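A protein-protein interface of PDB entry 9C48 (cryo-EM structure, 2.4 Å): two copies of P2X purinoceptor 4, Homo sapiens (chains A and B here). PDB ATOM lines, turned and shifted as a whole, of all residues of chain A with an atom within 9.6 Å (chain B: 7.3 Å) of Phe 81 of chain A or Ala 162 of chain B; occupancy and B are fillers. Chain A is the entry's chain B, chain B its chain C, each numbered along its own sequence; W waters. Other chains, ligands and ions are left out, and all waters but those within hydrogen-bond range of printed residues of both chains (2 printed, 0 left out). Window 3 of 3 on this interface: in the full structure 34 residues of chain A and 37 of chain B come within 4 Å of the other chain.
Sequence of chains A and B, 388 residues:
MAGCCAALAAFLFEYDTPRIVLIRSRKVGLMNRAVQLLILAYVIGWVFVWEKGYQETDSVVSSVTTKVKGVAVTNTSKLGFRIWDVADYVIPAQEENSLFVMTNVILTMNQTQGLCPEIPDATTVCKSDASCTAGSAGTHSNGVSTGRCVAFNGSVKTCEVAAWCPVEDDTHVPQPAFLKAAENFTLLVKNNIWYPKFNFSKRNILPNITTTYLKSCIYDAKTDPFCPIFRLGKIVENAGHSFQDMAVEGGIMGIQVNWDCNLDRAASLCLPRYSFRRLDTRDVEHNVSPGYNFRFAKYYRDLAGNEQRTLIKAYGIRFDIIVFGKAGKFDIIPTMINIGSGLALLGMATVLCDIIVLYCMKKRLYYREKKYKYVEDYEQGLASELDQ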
ATOM      1  N   GLY A  70      18.782 -24.009  23.360  1.00  0.00           N
ATOM      2  CA  GLY A  70      19.252 -22.665  23.071  1.00  0.00           C
ATOM      3  C   GLY A  70      20.481 -22.709  22.185  1.00  0.00           C
ATOM      4  O   GLY A  70      21.287 -23.637  22.240  1.00  0.00           O
ATOM      5  N   VAL A  71      20.629 -21.687  21.346  1.00  0.00           N
ATOM      6  CA  VAL A  71      21.738 -21.583  20.406  1.00  0.00           C
ATOM      7  C   VAL A  71      22.346 -20.190  20.513  1.00  0.00           C
ATOM      8  O   VAL A  71      21.624 -19.195  20.626  1.00  0.00           O
ATOM      9  CB  VAL A  71      21.290 -21.874  18.957  1.00  0.00           C
ATOM     10  CG1 VAL A  71      22.454 -21.745  17.996  1.00  0.00           C
ATOM     11  CG2 VAL A  71      20.686 -23.259  18.856  1.00  0.00           C
ATOM     12  N   ALA A  72      23.675 -20.123  20.484  1.00  0.00           N
ATOM     13  CA  ALA A  72      24.410 -18.867  20.505  1.00  0.00           C
ATOM     14  C   ALA A  72      25.266 -18.751  19.251  1.00  0.00           C
ATOM     15  O   ALA A  72      25.826 -19.743  18.781  1.00  0.00           O
ATOM     16  CB  ALA A  72      25.290 -18.763  21.752  1.00  0.00           C
ATOM     17  N   VAL A  73      25.365 -17.538  18.716  1.00  0.00           N
ATOM     18  CA  VAL A  73      26.137 -17.259  17.510  1.00  0.00           C
ATOM     19  C   VAL A  73      27.174 -16.193  17.830  1.00  0.00           C
ATOM     20  O   VAL A  73      26.844 -15.155  18.413  1.00  0.00           O
ATOM     21  CB  VAL A  73      25.236 -16.808  16.347  1.00  0.00           C
ATOM     22  CG1 VAL A  73      26.072 -16.483  15.127  1.00  0.00           C
ATOM     23  CG2 VAL A  73      24.228 -17.883  16.017  1.00  0.00           C
ATOM     24  N   THR A  74      28.424 -16.451  17.452  1.00  0.00           N
ATOM     25  CA  THR A  74      29.511 -15.498  17.616  1.00  0.00           C
ATOM     26  C   THR A  74      30.255 -15.351  16.295  1.00  0.00           C
ATOM     27  O   THR A  74      30.365 -16.300  15.521  1.00  0.00           O
ATOM     28  CB  THR A  74      30.492 -15.929  18.722  1.00  0.00           C
ATOM     29  OG1 THR A  74      31.099 -17.177  18.370  1.00  0.00           O
ATOM     30  CG2 THR A  74      29.771 -16.086  20.049  1.00  0.00           C
ATOM     31  N   ASN A  75      30.749 -14.143  16.041  1.00  0.00           N
ATOM     32  CA  ASN A  75      31.507 -13.810  14.836  1.00  0.00           C
ATOM     33  C   ASN A  75      32.744 -12.995  15.206  1.00  0.00           C
ATOM     34  O   ASN A  75      32.976 -11.896  14.700  1.00  0.00           O
ATOM     35  CB  ASN A  75      30.629 -13.074  13.823  1.00  0.00           C
ATOM     36  CG  ASN A  75      31.275 -12.961  12.441  1.00  0.00           C
ATOM     37  OD1 ASN A  75      32.493 -12.859  12.320  1.00  0.00           O
ATOM     38  ND2 ASN A  75      30.455 -12.966  11.394  1.00  0.00           N
ATOM     39  N   THR A  76      33.529 -13.504  16.150  1.00  0.00           N
ATOM     40  CA  THR A  76      34.777 -12.854  16.516  1.00  0.00           C
ATOM     41  C   THR A  76      35.812 -13.013  15.402  1.00  0.00           C
ATOM     42  O   THR A  76      35.692 -13.863  14.517  1.00  0.00           O
ATOM     43  CB  THR A  76      35.315 -13.421  17.827  1.00  0.00           C
ATOM     44  OG1 THR A  76      35.511 -14.834  17.694  1.00  0.00           O
ATOM     45  CG2 THR A  76      34.334 -13.154  18.955  1.00  0.00           C
ATOM     46  N   SER A  77      36.843 -12.169  15.452  1.00  0.00           N
ATOM     47  CA  SER A  77      37.853 -12.161  14.397  1.00  0.00           C
ATOM     48  C   SER A  77      38.770 -13.378  14.468  1.00  0.00           C
ATOM     49  O   SER A  77      39.122 -13.953  13.432  1.00  0.00           O
ATOM     50  CB  SER A  77      38.676 -10.876  14.469  1.00  0.00           C
ATOM     51  OG  SER A  77      37.856  -9.735  14.288  1.00  0.00           O
ATOM     52  N   LYS A  78      39.178 -13.776  15.675  1.00  0.00           N
ATOM     53  CA  LYS A  78      40.096 -14.904  15.811  1.00  0.00           C
ATOM     54  C   LYS A  78      39.407 -16.225  15.488  1.00  0.00           C
ATOM     55  O   LYS A  78      39.950 -17.054  14.750  1.00  0.00           O
ATOM     56  CB  LYS A  78      40.680 -14.932  17.223  1.00  0.00           C
ATOM     57  N   LEU A  79      38.212 -16.437  16.032  1.00  0.00           N
ATOM     58  CA  LEU A  79      37.491 -17.691  15.867  1.00  0.00           C
ATOM     59  C   LEU A  79      36.654 -17.743  14.598  1.00  0.00           C
ATOM     60  O   LEU A  79      36.224 -18.832  14.202  1.00  0.00           O
ATOM     61  CB  LEU A  79      36.579 -17.933  17.072  1.00  0.00           C
ATOM     62  CG  LEU A  79      37.034 -18.901  18.160  1.00  0.00           C
ATOM     63  CD1 LEU A  79      38.492 -18.676  18.514  1.00  0.00           C
ATOM     64  CD2 LEU A  79      36.150 -18.726  19.383  1.00  0.00           C
ATOM     65  N   GLY A  80      36.415 -16.608  13.949  1.00  0.00           N
ATOM     66  CA  GLY A  80      35.539 -16.605  12.791  1.00  0.00           C
ATOM     67  C   GLY A  80      34.088 -16.766  13.200  1.00  0.00           C
ATOM     68  O   GLY A  80      33.680 -16.392  14.304  1.00  0.00           O
ATOM     69  N   PHE A  81      33.295 -17.340  12.300  1.00  0.00           N
ATOM     70  CA  PHE A  81      31.875 -17.555  12.537  1.00  0.00           C
ATOM     71  C   PHE A  81      31.673 -18.901  13.218  1.00  0.00           C
ATOM     72  O   PHE A  81      32.111 -19.936  12.706  1.00  0.00           O
ATOM     73  CB  PHE A  81      31.103 -17.491  11.219  1.00  0.00           C
ATOM     74  CG  PHE A  81      29.628 -17.714  11.360  1.00  0.00           C
ATOM     75  CD1 PHE A  81      28.793 -16.679  11.741  1.00  0.00           C
ATOM     76  CD2 PHE A  81      29.070 -18.952  11.084  1.00  0.00           C
ATOM     77  CE1 PHE A  81      27.433 -16.878  11.864  1.00  0.00           C
ATOM     78  CE2 PHE A  81      27.712 -19.157  11.201  1.00  0.00           C
ATOM     79  CZ  PHE A  81      26.892 -18.118  11.593  1.00  0.00           C
ATOM     80  N   ARG A  82      31.022 -18.859  14.373  1.00  0.00           N
ATOM     81  CA  ARG A  82      30.818 -20.073  15.135  1.00  0.00           C
ATOM     82  C   ARG A  82      29.400 -20.243  15.621  1.00  0.00           C
ATOM     83  O   ARG A  82      28.698 -19.268  15.870  1.00  0.00           O
ATOM     84  CB  ARG A  82      31.765 -20.112  16.338  1.00  0.00           C
ATOM     85  CG  ARG A  82      33.242 -20.095  15.986  1.00  0.00           C
ATOM     86  CD  ARG A  82      33.657 -21.393  15.321  1.00  0.00           C
ATOM     87  NE  ARG A  82      33.254 -22.551  16.115  1.00  0.00           N
ATOM     88  CZ  ARG A  82      33.991 -23.092  17.079  1.00  0.00           C
ATOM     89  NH1 ARG A  82      35.179 -22.584  17.373  1.00  0.00           N
ATOM     90  NH2 ARG A  82      33.540 -24.144  17.748  1.00  0.00           N
ATOM     91  N   ILE A  83      28.976 -21.481  15.740  1.00  0.00           N
ATOM     92  CA  ILE A  83      27.650 -21.826  16.235  1.00  0.00           C
ATOM     93  C   ILE A  83      27.839 -22.646  17.500  1.00  0.00           C
ATOM     94  O   ILE A  83      28.678 -23.556  17.536  1.00  0.00           O
ATOM     95  CB  ILE A  83      26.836 -22.604  15.189  1.00  0.00           C
ATOM     96  CG1 ILE A  83      26.644 -21.771  13.921  1.00  0.00           C
ATOM     97  CG2 ILE A  83      25.484 -23.009  15.752  1.00  0.00           C
ATOM     98  CD1 ILE A  83      25.752 -20.578  14.107  1.00  0.00           C
ATOM     99  N   TRP A  84      27.087 -22.313  18.542  1.00  0.00           N
ATOM    100  CA  TRP A  84      27.137 -23.042  19.804  1.00  0.00           C
ATOM    101  C   TRP A  84      25.749 -23.591  20.096  1.00  0.00           C
ATOM    102  O   TRP A  84      24.824 -22.830  20.393  1.00  0.00           O
ATOM    103  CB  TRP A  84      27.638 -22.153  20.940  1.00  0.00           C
ATOM    104  CG  TRP A  84      28.921 -21.448  20.621  1.00  0.00           C
ATOM    105  CD1 TRP A  84      29.069 -20.295  19.911  1.00  0.00           C
ATOM    106  CD2 TRP A  84      30.239 -21.860  20.995  1.00  0.00           C
ATOM    107  NE1 TRP A  84      30.396 -19.962  19.820  1.00  0.00           N
ATOM    108  CE2 TRP A  84      31.136 -20.907  20.479  1.00  0.00           C
ATOM    109  CE3 TRP A  84      30.748 -22.942  21.720  1.00  0.00           C
ATOM    110  CZ2 TRP A  84      32.512 -21.002  20.665  1.00  0.00           C
ATOM    111  CZ3 TRP A  84      32.113 -23.033  21.903  1.00  0.00           C
ATOM    112  CH2 TRP A  84      32.979 -22.070  21.378  1.00  0.00           C
ATOM    113  N   ASP A  85      25.610 -24.906  20.009  1.00  0.00           N
ATOM    114  CA  ASP A  85      24.375 -25.611  20.307  1.00  0.00           C
ATOM    115  C   ASP A  85      24.588 -26.498  21.533  1.00  0.00           C
ATOM    116  O   ASP A  85      25.648 -26.476  22.160  1.00  0.00           O
ATOM    117  CB  ASP A  85      23.882 -26.360  19.060  1.00  0.00           C
ATOM    118  CG  ASP A  85      24.516 -27.736  18.872  1.00  0.00           C
ATOM    119  OD1 ASP A  85      25.508 -28.086  19.546  1.00  0.00           O
ATOM    120  OD2 ASP A  85      24.048 -28.461  17.974  1.00  0.00           O
ATOM    121  N   PHE A 178      31.784 -14.550  26.718  1.00  0.00           N
ATOM    122  CA  PHE A 178      31.765 -14.960  25.319  1.00  0.00           C
ATOM    123  C   PHE A 178      30.416 -15.550  24.932  1.00  0.00           C
ATOM    124  O   PHE A 178      29.909 -15.294  23.834  1.00  0.00           O
ATOM    125  CB  PHE A 178      32.892 -15.963  25.069  1.00  0.00           C
ATOM    126  CG  PHE A 178      33.151 -16.236  23.621  1.00  0.00           C
ATOM    127  CD1 PHE A 178      33.774 -15.292  22.829  1.00  0.00           C
ATOM    128  CD2 PHE A 178      32.784 -17.442  23.053  1.00  0.00           C
ATOM    129  CE1 PHE A 178      34.016 -15.541  21.500  1.00  0.00           C
ATOM    130  CE2 PHE A 178      33.026 -17.694  21.724  1.00  0.00           C
ATOM    131  CZ  PHE A 178      33.642 -16.743  20.946  1.00  0.00           C
ATOM    132  N   GLN B 113      29.391 -25.697  10.193  1.00  0.00           N
ATOM    133  CA  GLN B 113      28.756 -24.427  10.524  1.00  0.00           C
ATOM    134  C   GLN B 113      28.511 -23.601   9.266  1.00  0.00           C
ATOM    135  O   GLN B 113      29.424 -23.383   8.465  1.00  0.00           O
ATOM    136  CB  GLN B 113      29.619 -23.647  11.514  1.00  0.00           C
ATOM    137  CG  GLN B 113      29.650 -24.251  12.905  1.00  0.00           C
ATOM    138  CD  GLN B 113      30.959 -24.016  13.625  1.00  0.00           C
ATOM    139  OE1 GLN B 113      30.983 -23.479  14.729  1.00  0.00           O
ATOM    140  NE2 GLN B 113      32.059 -24.427  13.009  1.00  0.00           N
ATOM    141  N   GLY B 114      27.279 -23.129   9.104  1.00  0.00           N
ATOM    142  CA  GLY B 114      26.919 -22.388   7.905  1.00  0.00           C
ATOM    143  C   GLY B 114      25.445 -22.040   7.894  1.00  0.00           C
ATOM    144  O   GLY B 114      24.846 -21.779   8.941  1.00  0.00           O
ATOM    145  N   LEU B 115      24.874 -22.039   6.693  1.00  0.00           N
ATOM    146  CA  LEU B 115      23.472 -21.707   6.470  1.00  0.00           C
ATOM    147  C   LEU B 115      22.776 -22.865   5.768  1.00  0.00           C
ATOM    148  O   LEU B 115      23.326 -23.453   4.833  1.00  0.00           O
ATOM    149  CB  LEU B 115      23.336 -20.435   5.629  1.00  0.00           C
ATOM    150  CG  LEU B 115      23.955 -19.141   6.166  1.00  0.00           C
ATOM    151  CD1 LEU B 115      23.730 -18.011   5.182  1.00  0.00           C
ATOM    152  CD2 LEU B 115      23.387 -18.781   7.522  1.00  0.00           C
ATOM    153  N   CYS B 116      21.565 -23.187   6.215  1.00  0.00           N
ATOM    154  CA  CYS B 116      20.821 -24.315   5.672  1.00  0.00           C
ATOM    155  C   CYS B 116      19.342 -24.101   5.950  1.00  0.00           C
ATOM    156  O   CYS B 116      18.980 -23.344   6.857  1.00  0.00           O
ATOM    157  CB  CYS B 116      21.295 -25.643   6.286  1.00  0.00           C
ATOM    158  SG  CYS B 116      21.644 -25.574   8.052  1.00  0.00           S
ATOM    159  N   SER B 141      14.348 -23.950  18.083  1.00  0.00           N
ATOM    160  CA  SER B 141      15.096 -23.765  16.848  1.00  0.00           C
ATOM    161  C   SER B 141      16.551 -24.154  17.080  1.00  0.00           C
ATOM    162  O   SER B 141      17.209 -23.618  17.978  1.00  0.00           O
ATOM    163  CB  SER B 141      14.990 -22.319  16.371  1.00  0.00           C
ATOM    164  OG  SER B 141      15.602 -22.149  15.104  1.00  0.00           O
ATOM    165  N   ASN B 142      17.050 -25.095  16.274  1.00  0.00           N
ATOM    166  CA  ASN B 142      18.439 -25.524  16.379  1.00  0.00           C
ATOM    167  C   ASN B 142      19.410 -24.512  15.788  1.00  0.00           C
ATOM    168  O   ASN B 142      20.625 -24.704  15.900  1.00  0.00           O
ATOM    169  CB  ASN B 142      18.625 -26.885  15.705  1.00  0.00           C
ATOM    170  CG  ASN B 142      17.727 -27.065  14.500  1.00  0.00           C
ATOM    171  OD1 ASN B 142      17.314 -26.095  13.866  1.00  0.00           O
ATOM    172  ND2 ASN B 142      17.419 -28.314  14.177  1.00  0.00           N
ATOM    173  N   GLY B 143      18.911 -23.457  15.155  1.00  0.00           N
ATOM    174  CA  GLY B 143      19.753 -22.387  14.665  1.00  0.00           C
ATOM    175  C   GLY B 143      19.069 -21.044  14.780  1.00  0.00           C
ATOM    176  O   GLY B 143      17.946 -20.959  15.282  1.00  0.00           O
ATOM    177  N   VAL B 144      19.725 -19.987  14.318  1.00  0.00           N
ATOM    178  CA  VAL B 144      19.184 -18.633  14.378  1.00  0.00           C
ATOM    179  C   VAL B 144      18.699 -18.264  12.986  1.00  0.00           C
ATOM    180  O   VAL B 144      19.478 -18.270  12.026  1.00  0.00           O
ATOM    181  CB  VAL B 144      20.228 -17.630  14.893  1.00  0.00           C
ATOM    182  CG1 VAL B 144      19.669 -16.219  14.859  1.00  0.00           C
ATOM    183  CG2 VAL B 144      20.650 -17.995  16.302  1.00  0.00           C
ATOM    184  N   SER B 145      17.411 -17.944  12.876  1.00  0.00           N
ATOM    185  CA  SER B 145      16.812 -17.670  11.578  1.00  0.00           C
ATOM    186  C   SER B 145      17.387 -16.394  10.977  1.00  0.00           C
ATOM    187  O   SER B 145      17.566 -15.391  11.672  1.00  0.00           O
ATOM    188  CB  SER B 145      15.294 -17.559  11.714  1.00  0.00           C
ATOM    189  OG  SER B 145      14.699 -17.181  10.486  1.00  0.00           O
ATOM    190  N   THR B 146      17.681 -16.438   9.680  1.00  0.00           N
ATOM    191  CA  THR B 146      18.276 -15.313   8.974  1.00  0.00           C
ATOM    192  C   THR B 146      17.256 -14.466   8.228  1.00  0.00           C
ATOM    193  O   THR B 146      17.647 -13.517   7.538  1.00  0.00           O
ATOM    194  CB  THR B 146      19.342 -15.808   7.992  1.00  0.00           C
ATOM    195  OG1 THR B 146      18.711 -16.478   6.896  1.00  0.00           O
ATOM    196  CG2 THR B 146      20.292 -16.768   8.682  1.00  0.00           C
ATOM    197  N   GLU B 160      15.382 -20.247   6.478  1.00  0.00           N
ATOM    198  CA  GLU B 160      16.815 -20.485   6.583  1.00  0.00           C
ATOM    199  C   GLU B 160      17.314 -20.151   7.980  1.00  0.00           C
ATOM    200  O   GLU B 160      16.899 -19.158   8.584  1.00  0.00           O
ATOM    201  CB  GLU B 160      17.565 -19.650   5.548  1.00  0.00           C
ATOM    202  CG  GLU B 160      19.044 -19.963   5.445  1.00  0.00           C
ATOM    203  CD  GLU B 160      19.796 -18.924   4.651  1.00  0.00           C
ATOM    204  OE1 GLU B 160      20.362 -19.276   3.596  1.00  0.00           O
ATOM    205  OE2 GLU B 160      19.816 -17.753   5.078  1.00  0.00           O
ATOM    206  N   VAL B 161      18.219 -20.986   8.494  1.00  0.00           N
ATOM    207  CA  VAL B 161      18.806 -20.790   9.809  1.00  0.00           C
ATOM    208  C   VAL B 161      20.319 -20.912   9.702  1.00  0.00           C
ATOM    209  O   VAL B 161      20.859 -21.480   8.751  1.00  0.00           O
ATOM    210  CB  VAL B 161      18.266 -21.793  10.851  1.00  0.00           C
ATOM    211  CG1 VAL B 161      16.799 -21.531  11.130  1.00  0.00           C
ATOM    212  CG2 VAL B 161      18.482 -23.218  10.381  1.00  0.00           C
ATOM    213  N   ALA B 162      21.002 -20.359  10.700  1.00  0.00           N
ATOM    214  CA  ALA B 162      22.440 -20.520  10.857  1.00  0.00           C
ATOM    215  C   ALA B 162      22.692 -21.527  11.969  1.00  0.00           C
ATOM    216  O   ALA B 162      22.390 -21.253  13.135  1.00  0.00           O
ATOM    217  CB  ALA B 162      23.112 -19.184  11.175  1.00  0.00           C
ATOM    218  N   ALA B 163      23.235 -22.679  11.612  1.00  0.00           N
ATOM    219  CA  ALA B 163      23.474 -23.762  12.557  1.00  0.00           C
ATOM    220  C   ALA B 163      24.514 -24.692  11.947  1.00  0.00           C
ATOM    221  O   ALA B 163      25.149 -24.364  10.939  1.00  0.00           O
ATOM    222  CB  ALA B 163      22.179 -24.502  12.891  1.00  0.00           C
ATOM    223  N   TRP B 164      24.705 -25.849  12.575  1.00  0.00           N
ATOM    224  CA  TRP B 164      25.444 -26.931  11.946  1.00  0.00           C
ATOM    225  C   TRP B 164      24.567 -27.588  10.890  1.00  0.00           C
ATOM    226  O   TRP B 164      23.430 -27.974  11.170  1.00  0.00           O
ATOM    227  CB  TRP B 164      25.877 -27.955  12.990  1.00  0.00           C
ATOM    228  CG  TRP B 164      26.886 -27.461  13.980  1.00  0.00           C
ATOM    229  CD1 TRP B 164      26.639 -26.774  15.130  1.00  0.00           C
ATOM    230  CD2 TRP B 164      28.303 -27.661  13.932  1.00  0.00           C
ATOM    231  NE1 TRP B 164      27.812 -26.515  15.790  1.00  0.00           N
ATOM    232  CE2 TRP B 164      28.849 -27.053  15.078  1.00  0.00           C
ATOM    233  CE3 TRP B 164      29.163 -28.292  13.030  1.00  0.00           C
ATOM    234  CZ2 TRP B 164      30.214 -27.054  15.342  1.00  0.00           C
ATOM    235  CZ3 TRP B 164      30.515 -28.290  13.294  1.00  0.00           C
ATOM    236  CH2 TRP B 164      31.028 -27.679  14.439  1.00  0.00           C
ATOM    237  N   CYS B 165      25.092 -27.720   9.676  1.00  0.00           N
ATOM    238  CA  CYS B 165      24.279 -28.123   8.544  1.00  0.00           C
ATOM    239  C   CYS B 165      24.814 -29.405   7.920  1.00  0.00           C
ATOM    240  O   CYS B 165      26.032 -29.575   7.802  1.00  0.00           O
ATOM    241  CB  CYS B 165      24.240 -27.009   7.491  1.00  0.00           C
ATOM    242  SG  CYS B 165      23.667 -25.431   8.134  1.00  0.00           S
ATOM    243  N   VAL B 167      20.663 -29.952   9.150  1.00  0.00           N
ATOM    244  CA  VAL B 167      20.034 -30.086  10.456  1.00  0.00           C
ATOM    245  C   VAL B 167      19.530 -31.513  10.654  1.00  0.00           C
ATOM    246  O   VAL B 167      19.289 -32.260   9.706  1.00  0.00           O
ATOM    247  CB  VAL B 167      18.899 -29.062  10.631  1.00  0.00           C
ATOM    248  CG1 VAL B 167      19.452 -27.651  10.578  1.00  0.00           C
ATOM    249  CG2 VAL B 167      17.848 -29.251   9.563  1.00  0.00           C
ATOM    250  N   GLU B 307      36.118 -27.017  11.131  1.00  0.00           N
ATOM    251  CA  GLU B 307      35.526 -27.944  12.076  1.00  0.00           C
ATOM    252  C   GLU B 307      34.387 -28.725  11.462  1.00  0.00           C
ATOM    253  O   GLU B 307      33.575 -28.178  10.727  1.00  0.00           O
ATOM    254  CB  GLU B 307      35.044 -27.195  13.322  1.00  0.00           C
ATOM    255  CG  GLU B 307      34.631 -28.094  14.475  1.00  0.00           C
ATOM    256  CD  GLU B 307      34.278 -27.309  15.724  1.00  0.00           C
ATOM    257  OE1 GLU B 307      34.270 -26.063  15.662  1.00  0.00           O
ATOM    258  OE2 GLU B 307      34.010 -27.937  16.768  1.00  0.00           O
HETATM  259  O   HOH W   1      22.846 -26.482  15.469  1.00  0.00           O
HETATM  260  O   HOH W   2      32.498 -26.830  19.464  1.00  0.00           O
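The backbone NH (N) of Ile 83 of chain A lies within hydrogen-bond range of the side-chain amide oxygen (OE1) of Gln 113 of chain B, at 3.0 Å.
The guanidinium group (NE) of Arg 82 of chain A is in hydrogen-bond range of the side-chain amide oxygen (OE1) of Gln 113 of chain B.
OE1 of Glu 307 of chain B lies within salt-bridge range of NH2 of Arg 82 of chain A (2.9 Å).
N of Ala 162 of chain B is in hydrogen-bond range of O of Val 144 of chain B, 2.9 Å away.
The backbone carbonyl oxygen (O) of Thr 74 of chain A sits at hydrogen-bond distance from the backbone NH (N) of Arg 82 of chain A (2.9 Å).
N of Gly 114 of chain B is in hydrogen-bond range of O of Ala 163 of chain B, at 3.1 Å.
The side-chain sulfur of Cys 165 of chain B is disulfide-bonded to the side-chain sulfur of Cys 116 of chain B (2.0 Å).
O of Gly 143 of chain B sits at hydrogen-bond distance from OG of Ser 141 of chain B, 2.6 Å away.
Val 71 of chain A touches Ser 141 of chain B.
Val 71 of chain A touches Asn 142 of chain B.
Val 73 of chain A touches Val 144 of chain B.
Phe 81 of chain A touches Ala 162 of chain B.
CD1 of Ile 83 of chain A touches O of Ala 162 of chain B, at 3.6 Å.
Ile 83 of chain A touches Ala 163 of chain B (CG2 to CA, 3.8 Å).
Trp 164 of chain B touches Ile 83 of chain A (NE1 to O, 3.5 Å).
Of the printed residues of chain B, Val 71 of chain A touches Ser 141 (3.6 Å) and Asn 142 (3.3 Å).
Thr 76 of chain A touches none of the printed residues of chain B.
Phe 81 of chain A touches just one residue of chain B: Ala 162.
Of the printed residues of chain B, Ile 83 of chain A touches Gln 113, Ala 162, Ala 163 and Trp 164.
Of the printed residues of chain A, Gln 113 of chain B touches Arg 82 and Ile 83.
Printed residues of chain A within 4 Å of Ser 141 of chain B: Val 71 (3.6 Å).
Of the printed residues of chain A, Val 144 of chain B touches Val 73.
No residue of chain A comes within 4 Å of Val 161 of chain B.
Of the printed residues of chain A, Ala 162 of chain B touches Phe 81 (3.9 Å) and Ile 83 (3.6 Å).
Of chain A, only Ile 83 (3.8 Å) comes within 4 Å of Ala 163 of chain B.
The nearest residue of chain A that does not touch Ala 162 of chain B is Val 73 of chain A (4.8 Å).
Of the 18 printed residues of chain B, 8 touch a printed residue of chain A.
Hydrophobic or aromatic side chains of chain B within 4 Å of the printed part of chain A: Val 144, Ala 162 and Trp 164.
Among the printed residues, 10 pairs touch across the chains.
No position is printed for both chains.
Of the 10 pairs that touch across the chains among the printed residues, none has its exchanged pair printed and touching as well.
Water W1 lies within hydrogen-bond range of O of Asn 142 of chain B (2.9 Å), OD2 of Asp 85 of chain A (3.4 Å) and N of Trp 164 of chain B (3.5 Å).
Water W2 lies within hydrogen-bond range of the side-chain carboxylate of Glu 307 of chain B (3.3 Å) and the guanidinium group of Arg 82 of chain A (3.4 Å).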
